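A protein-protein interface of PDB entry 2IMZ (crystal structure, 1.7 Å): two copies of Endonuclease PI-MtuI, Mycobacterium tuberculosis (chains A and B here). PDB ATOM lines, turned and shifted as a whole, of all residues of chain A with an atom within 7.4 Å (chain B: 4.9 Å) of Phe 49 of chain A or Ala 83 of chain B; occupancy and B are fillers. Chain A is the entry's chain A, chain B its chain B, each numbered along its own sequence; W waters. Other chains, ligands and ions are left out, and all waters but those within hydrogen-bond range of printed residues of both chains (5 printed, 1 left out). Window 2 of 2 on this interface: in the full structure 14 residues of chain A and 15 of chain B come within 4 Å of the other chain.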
ATOM      1  N   CSD A   1      -3.611  14.550 -28.431  1.00  0.00           N
ATOM      2  CA  CSD A   1      -3.750  13.172 -29.005  1.00  0.00           C
ATOM      3  CB  CSD A   1      -5.002  12.495 -28.454  1.00  0.00           C
ATOM      4  SG  CSD A   1      -4.973  12.410 -26.638  1.00  0.00           S
ATOM      5  C   CSD A   1      -3.818  13.202 -30.527  1.00  0.00           C
ATOM      6  O   CSD A   1      -4.283  14.175 -31.125  1.00  0.00           O
ATOM      7  OD1 CSD A   1      -3.691  11.808 -26.247  1.00  0.00           O
ATOM      8  OD2 CSD A   1      -5.029  13.791 -26.124  1.00  0.00           O
ATOM      9  N   LEU A   2      -3.362  12.121 -31.150  1.00  0.00           N
ATOM     10  CA  LEU A   2      -3.345  12.028 -32.604  1.00  0.00           C
ATOM     11  C   LEU A   2      -4.436  11.090 -33.105  1.00  0.00           C
ATOM     12  O   LEU A   2      -4.681  10.039 -32.524  1.00  0.00           O
ATOM     13  CB  LEU A   2      -1.959  11.551 -33.067  1.00  0.00           C
ATOM     14  CG  LEU A   2      -0.784  12.401 -32.550  1.00  0.00           C
ATOM     15  CD1 LEU A   2       0.540  11.761 -32.938  1.00  0.00           C
ATOM     16  CD2 LEU A   2      -0.870  13.823 -33.114  1.00  0.00           C
ATOM     17  N   ILE A  19      -0.625   5.082 -36.604  1.00  0.00           N
ATOM     18  CA  ILE A  19      -0.523   5.098 -35.155  1.00  0.00           C
ATOM     19  C   ILE A  19      -1.384   4.063 -34.424  1.00  0.00           C
ATOM     20  O   ILE A  19      -0.945   3.494 -33.423  1.00  0.00           O
ATOM     21  CB  ILE A  19      -0.811   6.518 -34.595  1.00  0.00           C
ATOM     22  CG1 ILE A  19      -0.360   6.592 -33.133  1.00  0.00           C
ATOM     23  CG2 ILE A  19      -2.293   6.863 -34.740  1.00  0.00           C
ATOM     24  CD1 ILE A  19      -0.192   8.018 -32.608  1.00  0.00           C
ATOM     25  N   VAL A  22       0.380   0.818 -34.321  1.00  0.00           N
ATOM     26  CA  VAL A  22       1.511   0.866 -33.410  1.00  0.00           C
ATOM     27  C   VAL A  22       1.024   0.665 -31.979  1.00  0.00           C
ATOM     28  O   VAL A  22       1.637  -0.069 -31.206  1.00  0.00           O
ATOM     29  CB  VAL A  22       2.247   2.221 -33.515  1.00  0.00           C
ATOM     30  CG1 VAL A  22       3.391   2.281 -32.522  1.00  0.00           C
ATOM     31  CG2 VAL A  22       2.780   2.403 -34.927  1.00  0.00           C
ATOM     32  N   VAL A  23      -0.083   1.313 -31.632  1.00  0.00           N
ATOM     33  CA  VAL A  23      -0.636   1.192 -30.284  1.00  0.00           C
ATOM     34  C   VAL A  23      -1.295  -0.169 -30.038  1.00  0.00           C
ATOM     35  O   VAL A  23      -1.068  -0.788 -28.993  1.00  0.00           O
ATOM     36  CB  VAL A  23      -1.664   2.317 -30.000  1.00  0.00           C
ATOM     37  CG1 VAL A  23      -2.392   2.046 -28.687  1.00  0.00           C
ATOM     38  CG2 VAL A  23      -0.944   3.662 -29.922  1.00  0.00           C
ATOM     39  N   ASP A  24      -2.100  -0.637 -30.988  1.00  0.00           N
ATOM     40  CA  ASP A  24      -2.776  -1.929 -30.830  1.00  0.00           C
ATOM     41  C   ASP A  24      -1.782  -3.077 -30.683  1.00  0.00           C
ATOM     42  O   ASP A  24      -2.047  -4.052 -29.974  1.00  0.00           O
ATOM     43  CB  ASP A  24      -3.704  -2.220 -32.015  1.00  0.00           C
ATOM     44  CG  ASP A  24      -4.842  -1.222 -32.133  1.00  0.00           C
ATOM     45  OD1 ASP A  24      -5.301  -0.699 -31.094  1.00  0.00           O
ATOM     46  OD2 ASP A  24      -5.290  -0.970 -33.272  1.00  0.00           O
ATOM     47  N   VAL A  45       9.931   3.940 -29.366  1.00  0.00           N
ATOM     48  CA  VAL A  45       8.672   4.172 -28.676  1.00  0.00           C
ATOM     49  C   VAL A  45       8.720   3.227 -27.478  1.00  0.00           C
ATOM     50  O   VAL A  45       9.052   2.050 -27.634  1.00  0.00           O
ATOM     51  CB  VAL A  45       7.472   3.811 -29.574  1.00  0.00           C
ATOM     52  CG1 VAL A  45       6.170   3.888 -28.781  1.00  0.00           C
ATOM     53  CG2 VAL A  45       7.420   4.770 -30.763  1.00  0.00           C
ATOM     54  N   VAL A  46       8.405   3.743 -26.293  1.00  0.00           N
ATOM     55  CA  VAL A  46       8.446   2.940 -25.074  1.00  0.00           C
ATOM     56  C   VAL A  46       7.104   2.789 -24.362  1.00  0.00           C
ATOM     57  O   VAL A  46       6.966   1.959 -23.461  1.00  0.00           O
ATOM     58  CB  VAL A  46       9.488   3.508 -24.088  1.00  0.00           C
ATOM     59  CG1 VAL A  46      10.884   3.350 -24.677  1.00  0.00           C
ATOM     60  CG2 VAL A  46       9.204   4.974 -23.804  1.00  0.00           C
ATOM     61  N   SER A  47       6.120   3.587 -24.764  1.00  0.00           N
ATOM     62  CA  SER A  47       4.780   3.523 -24.177  1.00  0.00           C
ATOM     63  C   SER A  47       3.743   3.747 -25.267  1.00  0.00           C
ATOM     64  O   SER A  47       3.992   4.479 -26.228  1.00  0.00           O
ATOM     65  CB  SER A  47       4.603   4.581 -23.085  1.00  0.00           C
ATOM     66  OG  SER A  47       5.522   4.394 -22.028  1.00  0.00           O
ATOM     67  N   TRP A  48       2.577   3.126 -25.100  1.00  0.00           N
ATOM     68  CA  TRP A  48       1.489   3.209 -26.074  1.00  0.00           C
ATOM     69  C   TRP A  48       0.177   3.563 -25.382  1.00  0.00           C
ATOM     70  O   TRP A  48      -0.176   2.958 -24.366  1.00  0.00           O
ATOM     71  CB  TRP A  48       1.336   1.857 -26.778  1.00  0.00           C
ATOM     72  CG  TRP A  48       2.599   1.373 -27.410  1.00  0.00           C
ATOM     73  CD1 TRP A  48       2.996   1.565 -28.700  1.00  0.00           C
ATOM     74  CD2 TRP A  48       3.666   0.674 -26.760  1.00  0.00           C
ATOM     75  NE1 TRP A  48       4.246   1.033 -28.896  1.00  0.00           N
ATOM     76  CE2 TRP A  48       4.683   0.480 -27.721  1.00  0.00           C
ATOM     77  CE3 TRP A  48       3.865   0.197 -25.456  1.00  0.00           C
ATOM     78  CZ2 TRP A  48       5.884  -0.175 -27.422  1.00  0.00           C
ATOM     79  CZ3 TRP A  48       5.061  -0.455 -25.157  1.00  0.00           C
ATOM     80  CH2 TRP A  48       6.055  -0.633 -26.139  1.00  0.00           C
ATOM     81  N   PHE A  49      -0.559   4.522 -25.938  1.00  0.00           N
ATOM     82  CA  PHE A  49      -1.826   4.922 -25.336  1.00  0.00           C
ATOM     83  C   PHE A  49      -3.002   5.003 -26.303  1.00  0.00           C
ATOM     84  O   PHE A  49      -2.915   5.637 -27.356  1.00  0.00           O
ATOM     85  CB  PHE A  49      -1.676   6.274 -24.631  1.00  0.00           C
ATOM     86  CG  PHE A  49      -0.505   6.344 -23.696  1.00  0.00           C
ATOM     87  CD1 PHE A  49       0.763   6.667 -24.171  1.00  0.00           C
ATOM     88  CD2 PHE A  49      -0.662   6.056 -22.343  1.00  0.00           C
ATOM     89  CE1 PHE A  49       1.862   6.701 -23.311  1.00  0.00           C
ATOM     90  CE2 PHE A  49       0.431   6.087 -21.473  1.00  0.00           C
ATOM     91  CZ  PHE A  49       1.695   6.410 -21.962  1.00  0.00           C
ATOM     92  N   ASP A  50      -4.094   4.333 -25.945  1.00  0.00           N
ATOM     93  CA  ASP A  50      -5.323   4.369 -26.734  1.00  0.00           C
ATOM     94  C   ASP A  50      -6.142   5.398 -25.963  1.00  0.00           C
ATOM     95  O   ASP A  50      -6.646   5.110 -24.879  1.00  0.00           O
ATOM     96  CB  ASP A  50      -6.030   3.013 -26.714  1.00  0.00           C
ATOM     97  CG  ASP A  50      -7.286   2.997 -27.567  1.00  0.00           C
ATOM     98  OD1 ASP A  50      -8.057   3.978 -27.515  1.00  0.00           O
ATOM     99  OD2 ASP A  50      -7.511   1.999 -28.282  1.00  0.00           O
ATOM    100  N   GLN A  51      -6.265   6.594 -26.526  1.00  0.00           N
ATOM    101  CA  GLN A  51      -6.955   7.695 -25.868  1.00  0.00           C
ATOM    102  C   GLN A  51      -8.457   7.833 -26.087  1.00  0.00           C
ATOM    103  O   GLN A  51      -9.062   8.802 -25.623  1.00  0.00           O
ATOM    104  CB  GLN A  51      -6.264   9.005 -26.253  1.00  0.00           C
ATOM    105  CG  GLN A  51      -4.750   8.977 -26.074  1.00  0.00           C
ATOM    106  CD  GLN A  51      -4.324   8.882 -24.621  1.00  0.00           C
ATOM    107  OE1 GLN A  51      -3.599   9.742 -24.119  1.00  0.00           O
ATOM    108  NE2 GLN A  51      -4.769   7.836 -23.938  1.00  0.00           N
ATOM    109  N   GLY A  52      -9.058   6.877 -26.788  1.00  0.00           N
ATOM    110  CA  GLY A  52     -10.488   6.937 -27.033  1.00  0.00           C
ATOM    111  C   GLY A  52     -10.886   7.955 -28.085  1.00  0.00           C
ATOM    112  O   GLY A  52     -10.032   8.595 -28.700  1.00  0.00           O
ATOM    113  N   THR A 148      -8.452   8.407 -31.022  1.00  0.00           N
ATOM    114  CA  THR A 148      -7.151   9.049 -30.914  1.00  0.00           C
ATOM    115  C   THR A 148      -6.151   8.212 -30.133  1.00  0.00           C
ATOM    116  O   THR A 148      -6.527   7.313 -29.374  1.00  0.00           O
ATOM    117  CB  THR A 148      -7.283  10.445 -30.274  1.00  0.00           C
ATOM    118  OG1 THR A 148      -7.811  10.321 -28.948  1.00  0.00           O
ATOM    119  CG2 THR A 148      -8.216  11.314 -31.105  1.00  0.00           C
ATOM    120  N   PHE A 149      -4.871   8.517 -30.328  1.00  0.00           N
ATOM    121  CA  PHE A 149      -3.795   7.775 -29.693  1.00  0.00           C
ATOM    122  C   PHE A 149      -2.618   8.664 -29.334  1.00  0.00           C
ATOM    123  O   PHE A 149      -2.546   9.822 -29.748  1.00  0.00           O
ATOM    124  CB  PHE A 149      -3.305   6.669 -30.631  1.00  0.00           C
ATOM    125  CG  PHE A 149      -4.406   5.817 -31.187  1.00  0.00           C
ATOM    126  CD1 PHE A 149      -5.174   6.260 -32.259  1.00  0.00           C
ATOM    127  CD2 PHE A 149      -4.712   4.593 -30.603  1.00  0.00           C
ATOM    128  CE1 PHE A 149      -6.235   5.500 -32.742  1.00  0.00           C
ATOM    129  CE2 PHE A 149      -5.767   3.825 -31.077  1.00  0.00           C
ATOM    130  CZ  PHE A 149      -6.534   4.279 -32.149  1.00  0.00           C
ATOM    131  N   ASP A 150      -1.682   8.098 -28.583  1.00  0.00           N
ATOM    132  CA  ASP A 150      -0.494   8.822 -28.160  1.00  0.00           C
ATOM    133  C   ASP A 150       0.654   7.824 -28.004  1.00  0.00           C
ATOM    134  O   ASP A 150       0.422   6.632 -27.802  1.00  0.00           O
ATOM    135  CB  ASP A 150      -0.778   9.530 -26.831  1.00  0.00           C
ATOM    136  CG  ASP A 150       0.127  10.716 -26.592  1.00  0.00           C
ATOM    137  OD1 ASP A 150       0.284  11.544 -27.516  1.00  0.00           O
ATOM    138  OD2 ASP A 150       0.668  10.833 -25.469  1.00  0.00           O
ATOM    139  N   LEU A 151       1.884   8.313 -28.112  1.00  0.00           N
ATOM    140  CA  LEU A 151       3.066   7.464 -27.981  1.00  0.00           C
ATOM    141  C   LEU A 151       4.124   8.153 -27.133  1.00  0.00           C
ATOM    142  O   LEU A 151       4.230   9.377 -27.149  1.00  0.00           O
ATOM    143  CB  LEU A 151       3.674   7.179 -29.359  1.00  0.00           C
ATOM    144  CG  LEU A 151       2.826   6.469 -30.415  1.00  0.00           C
ATOM    145  CD1 LEU A 151       3.540   6.516 -31.769  1.00  0.00           C
ATOM    146  CD2 LEU A 151       2.577   5.026 -29.984  1.00  0.00           C
ATOM    147  N   GLU A 152       4.893   7.370 -26.380  1.00  0.00           N
ATOM    148  CA  GLU A 152       5.984   7.929 -25.593  1.00  0.00           C
ATOM    149  C   GLU A 152       7.267   7.518 -26.288  1.00  0.00           C
ATOM    150  O   GLU A 152       7.476   6.337 -26.578  1.00  0.00           O
ATOM    151  CB  GLU A 152       5.999   7.404 -24.156  1.00  0.00           C
ATOM    152  CG  GLU A 152       5.135   8.196 -23.192  1.00  0.00           C
ATOM    153  CD  GLU A 152       5.452   9.688 -23.192  1.00  0.00           C
ATOM    154  OE1 GLU A 152       6.612  10.085 -22.918  1.00  0.00           O
ATOM    155  OE2 GLU A 152       4.528  10.469 -23.470  1.00  0.00           O
ATOM    156  N   VAL A 153       8.107   8.509 -26.559  1.00  0.00           N
ATOM    157  CA  VAL A 153       9.383   8.317 -27.232  1.00  0.00           C
ATOM    158  C   VAL A 153      10.500   8.520 -26.220  1.00  0.00           C
ATOM    159  O   VAL A 153      10.602   9.571 -25.589  1.00  0.00           O
ATOM    160  CB  VAL A 153       9.547   9.331 -28.390  1.00  0.00           C
ATOM    161  CG1 VAL A 153      10.908   9.163 -29.056  1.00  0.00           C
ATOM    162  CG2 VAL A 153       8.434   9.128 -29.410  1.00  0.00           C
ATOM    163  N   PRO B  71      -7.072  12.140 -15.902  1.00  0.00           N
ATOM    164  CA  PRO B  71      -6.809  10.708 -16.068  1.00  0.00           C
ATOM    165  C   PRO B  71      -5.742  10.392 -17.116  1.00  0.00           C
ATOM    166  O   PRO B  71      -5.022   9.401 -16.992  1.00  0.00           O
ATOM    167  CB  PRO B  71      -8.181  10.150 -16.444  1.00  0.00           C
ATOM    168  CG  PRO B  71      -9.121  11.060 -15.704  1.00  0.00           C
ATOM    169  CD  PRO B  71      -8.518  12.424 -15.949  1.00  0.00           C
ATOM    170  N   ASP B  72      -5.632  11.229 -18.142  1.00  0.00           N
ATOM    171  CA  ASP B  72      -4.644  10.971 -19.181  1.00  0.00           C
ATOM    172  C   ASP B  72      -3.265  11.573 -18.912  1.00  0.00           C
ATOM    173  O   ASP B  72      -2.342  11.404 -19.713  1.00  0.00           O
ATOM    174  CB  ASP B  72      -5.169  11.426 -20.552  1.00  0.00           C
ATOM    175  CG  ASP B  72      -5.550  12.892 -20.592  1.00  0.00           C
ATOM    176  OD1 ASP B  72      -6.156  13.310 -21.604  1.00  0.00           O
ATOM    177  OD2 ASP B  72      -5.252  13.629 -19.631  1.00  0.00           O
ATOM    178  N   HIS B  73      -3.108  12.267 -17.788  1.00  0.00           N
ATOM    179  CA  HIS B  73      -1.803  12.841 -17.494  1.00  0.00           C
ATOM    180  C   HIS B  73      -0.829  11.715 -17.181  1.00  0.00           C
ATOM    181  O   HIS B  73      -1.143  10.801 -16.417  1.00  0.00           O
ATOM    182  CB  HIS B  73      -1.846  13.802 -16.310  1.00  0.00           C
ATOM    183  CG  HIS B  73      -0.681  14.739 -16.276  1.00  0.00           C
ATOM    184  ND1 HIS B  73      -0.700  15.965 -16.906  1.00  0.00           N
ATOM    185  CD2 HIS B  73       0.577  14.582 -15.798  1.00  0.00           C
ATOM    186  CE1 HIS B  73       0.497  16.520 -16.824  1.00  0.00           C
ATOM    187  NE2 HIS B  73       1.291  15.700 -16.159  1.00  0.00           N
ATOM    188  N   LYS B  74       0.361  11.786 -17.766  1.00  0.00           N
ATOM    189  CA  LYS B  74       1.360  10.748 -17.550  1.00  0.00           C
ATOM    190  C   LYS B  74       2.199  10.953 -16.297  1.00  0.00           C
ATOM    191  O   LYS B  74       2.659  12.058 -16.001  1.00  0.00           O
ATOM    192  CB  LYS B  74       2.246  10.627 -18.791  1.00  0.00           C
ATOM    193  CG  LYS B  74       1.497   9.992 -19.960  1.00  0.00           C
ATOM    194  CD  LYS B  74       2.212  10.161 -21.290  1.00  0.00           C
ATOM    195  CE  LYS B  74       2.128  11.605 -21.763  1.00  0.00           C
ATOM    196  NZ  LYS B  74       2.442  11.752 -23.213  1.00  0.00           N
ATOM    197  N   TRP B  81       6.299   5.372 -18.103  1.00  0.00           N
ATOM    198  CA  TRP B  81       5.208   6.333 -18.160  1.00  0.00           C
ATOM    199  C   TRP B  81       3.856   5.647 -18.280  1.00  0.00           C
ATOM    200  O   TRP B  81       3.643   4.816 -19.164  1.00  0.00           O
ATOM    201  CB  TRP B  81       5.406   7.300 -19.331  1.00  0.00           C
ATOM    202  CG  TRP B  81       6.633   8.139 -19.189  1.00  0.00           C
ATOM    203  CD1 TRP B  81       7.830   7.965 -19.826  1.00  0.00           C
ATOM    204  CD2 TRP B  81       6.806   9.254 -18.308  1.00  0.00           C
ATOM    205  NE1 TRP B  81       8.737   8.903 -19.395  1.00  0.00           N
ATOM    206  CE2 TRP B  81       8.134   9.708 -18.463  1.00  0.00           C
ATOM    207  CE3 TRP B  81       5.965   9.914 -17.401  1.00  0.00           C
ATOM    208  CZ2 TRP B  81       8.644  10.794 -17.741  1.00  0.00           C
ATOM    209  CZ3 TRP B  81       6.472  10.996 -16.683  1.00  0.00           C
ATOM    210  CH2 TRP B  81       7.799  11.423 -16.860  1.00  0.00           C
ATOM    211  N   ARG B  82       2.942   6.002 -17.383  1.00  0.00           N
ATOM    212  CA  ARG B  82       1.598   5.435 -17.386  1.00  0.00           C
ATOM    213  C   ARG B  82       0.608   6.565 -17.136  1.00  0.00           C
ATOM    214  O   ARG B  82       0.946   7.562 -16.494  1.00  0.00           O
ATOM    215  CB  ARG B  82       1.451   4.387 -16.278  1.00  0.00           C
ATOM    216  CG  ARG B  82       2.535   3.321 -16.267  1.00  0.00           C
ATOM    217  CD  ARG B  82       2.541   2.518 -17.553  1.00  0.00           C
ATOM    218  NE  ARG B  82       3.893   2.405 -18.094  1.00  0.00           N
ATOM    219  CZ  ARG B  82       4.184   1.859 -19.269  1.00  0.00           C
ATOM    220  NH1 ARG B  82       3.214   1.369 -20.028  1.00  0.00           N
ATOM    221  NH2 ARG B  82       5.440   1.819 -19.692  1.00  0.00           N
ATOM    222  N   ALA B  83      -0.611   6.411 -17.642  1.00  0.00           N
ATOM    223  CA  ALA B  83      -1.644   7.425 -17.451  1.00  0.00           C
ATOM    224  C   ALA B  83      -2.155   7.337 -16.016  1.00  0.00           C
ATOM    225  O   ALA B  83      -2.388   6.245 -15.501  1.00  0.00           O
ATOM    226  CB  ALA B  83      -2.794   7.204 -18.438  1.00  0.00           C
ATOM    227  N   ALA B  84      -2.321   8.492 -15.376  1.00  0.00           N
ATOM    228  CA  ALA B  84      -2.795   8.550 -13.997  1.00  0.00           C
ATOM    229  C   ALA B  84      -4.057   7.711 -13.803  1.00  0.00           C
ATOM    230  O   ALA B  84      -4.229   7.055 -12.772  1.00  0.00           O
ATOM    231  CB  ALA B  84      -3.065  10.000 -13.608  1.00  0.00           C
ATOM    232  N   GLY B  85      -4.933   7.741 -14.800  1.00  0.00           N
ATOM    233  CA  GLY B  85      -6.174   6.990 -14.726  1.00  0.00           C
ATOM    234  C   GLY B  85      -6.007   5.483 -14.791  1.00  0.00           C
ATOM    235  O   GLY B  85      -6.937   4.747 -14.466  1.00  0.00           O
ATOM    236  N   GLU B  86      -4.831   5.022 -15.212  1.00  0.00           N
ATOM    237  CA  GLU B  86      -4.545   3.589 -15.317  1.00  0.00           C
ATOM    238  C   GLU B  86      -3.973   3.022 -14.019  1.00  0.00           C
ATOM    239  O   GLU B  86      -3.941   1.805 -13.827  1.00  0.00           O
ATOM    240  CB  GLU B  86      -3.530   3.320 -16.433  1.00  0.00           C
ATOM    241  CG  GLU B  86      -3.936   3.779 -17.820  1.00  0.00           C
ATOM    242  CD  GLU B  86      -2.858   3.502 -18.859  1.00  0.00           C
ATOM    243  OE1 GLU B  86      -1.737   4.049 -18.739  1.00  0.00           O
ATOM    244  OE2 GLU B  86      -3.132   2.730 -19.801  1.00  0.00           O
ATOM    245  N   LEU B  87      -3.513   3.905 -13.139  1.00  0.00           N
ATOM    246  CA  LEU B  87      -2.911   3.486 -11.878  1.00  0.00           C
ATOM    247  C   LEU B  87      -3.925   3.157 -10.787  1.00  0.00           C
ATOM    248  O   LEU B  87      -5.018   3.722 -10.742  1.00  0.00           O
ATOM    249  CB  LEU B  87      -1.945   4.571 -11.392  1.00  0.00           C
ATOM    250  CG  LEU B  87      -0.869   4.945 -12.417  1.00  0.00           C
ATOM    251  CD1 LEU B  87      -0.006   6.077 -11.875  1.00  0.00           C
ATOM    252  CD2 LEU B  87      -0.015   3.721 -12.738  1.00  0.00           C
HETATM  253  O   HOH W   1       7.709   4.548 -20.566  1.00  0.00           O
HETATM  254  O   HOH W   2       5.013   0.559 -21.958  1.00  0.00           O
HETATM  255  O   HOH W   3      -2.155   9.468 -21.562  1.00  0.00           O
HETATM  256  O   HOH W   4       2.247   1.676 -22.397  1.00  0.00           O
HETATM  257  O   HOH W   5      -4.047  14.020 -23.453  1.00  0.00           O
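No position is printed for both chains. Of the 8 pairs that touch across the chains among the printed residues, none has its exchanged pair printed and touching as well.
Among the printed residues, merely in contact across the chains: Phe 49 of chain A with Trp 81 of chain B (3.8 Å), Phe 49 of chain A with Lys 74 of chain B (3.8 Å), Glu 152 of chain A with Trp 81 of chain B (3.9 Å) and Phe 49 of chain A with Ala 83 of chain B (3.98 Å).
The backbone carbonyl oxygen (O) of Asp 150 of chain A lies within hydrogen-bond range of the backbone NH (N) of Phe 49 of chain A (3.0 Å). OE1 of Glu 86 of chain B lies within hydrogen-bond range of N of Ala 83 of chain B. O of Ser 47 of chain A is in hydrogen-bond range of N of Glu 152 of chain A (3.0 Å). The backbone carbonyl oxygen of Glu 152 of chain A is in hydrogen-bond range of the backbone NH of Val 46 of chain A.
Ile 19 of chain A touches none of the printed residues of chain B. Of the printed residues of chain B, Phe 49 of chain A touches Lys 74 (3.8 Å), Trp 81 (3.8 Å) and Ala 83 (3.98 Å). Of the printed residues of chain B, Asp 150 of chain A touches Lys 74 (3.0 Å). Printed residues of chain B within 4 Å of Glu 152 of chain A: Lys 74 and Trp 81. Of the printed residues of chain A, Lys 74 of chain B touches Phe 49, Asp 150 and Glu 152. Printed residues of chain A within 4 Å of Arg 82 of chain B: Ser 47 (3.5 Å). Gly 85 of chain B touches none of the printed residues of chain A. The nearest printed residue of chain A that does not touch Ala 83 of chain B is Gln 51 of chain A (5.9 Å). The nearest printed residue of chain A that does not touch Arg 82 of chain B is Val 46 of chain A (4.1 Å).
Of the 20 printed residues of chain A, 4 touch a printed residue of chain B. Hydrophobic or aromatic side chains of chain A that line the printed part of chain B: Phe 49. Along chain A the printed residues that touch a printed residue of chain B span positions 47 to 152. Among the printed residues, 8 pairs touch across the chains. Among the printed residues, Asp or Glu carboxylates within 4 Å of a Lys or Arg side-chain nitrogen of the other chain: Asp 150 of chain A with Lys 74 of chain B (3.0 Å) and Glu 152 of chain A with Lys 74 of chain B (2.5 Å).
OG of Ser 47 of chain A sits at hydrogen-bond distance from O of Trp 81 of chain B (3.5 Å). The side-chain carboxylate of Asp 150 of chain A lies within salt-bridge range of the side-chain amino group of Lys 74 of chain B, 3.0 Å away. The side-chain carboxylate (OE2) of Glu 152 of chain A is in salt-bridge range of the side-chain amino group (NZ) of Lys 74 of chain B, 2.5 Å away. The side-chain hydroxyl (OG) of Ser 47 of chain A sits at hydrogen-bond distance from the guanidinium group (NH2) of Arg 82 of chain B (3.5 Å).
Water W4 bridges the guanidinium group of Arg 82 of chain B (2.6 Å) and the backbone NH of Trp 48 of chain A (3.1 Å). Water W2 bridges NH2 of Arg 82 of chain B (2.6 Å) and O of Val 46 of chain A (2.8 Å). Water W1 lies within hydrogen-bond range of OG of Ser 47 of chain A (2.6 Å) and N of Trp 81 of chain B (3.0 Å). Water W3 bridges O of Asp 72 of chain B and OE1 of Gln 51 of chain A. Water W5 lies within hydrogen-bond range of OD2 of CSD 1 of chain A and the side-chain carboxylate of Asp 72 of chain B.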
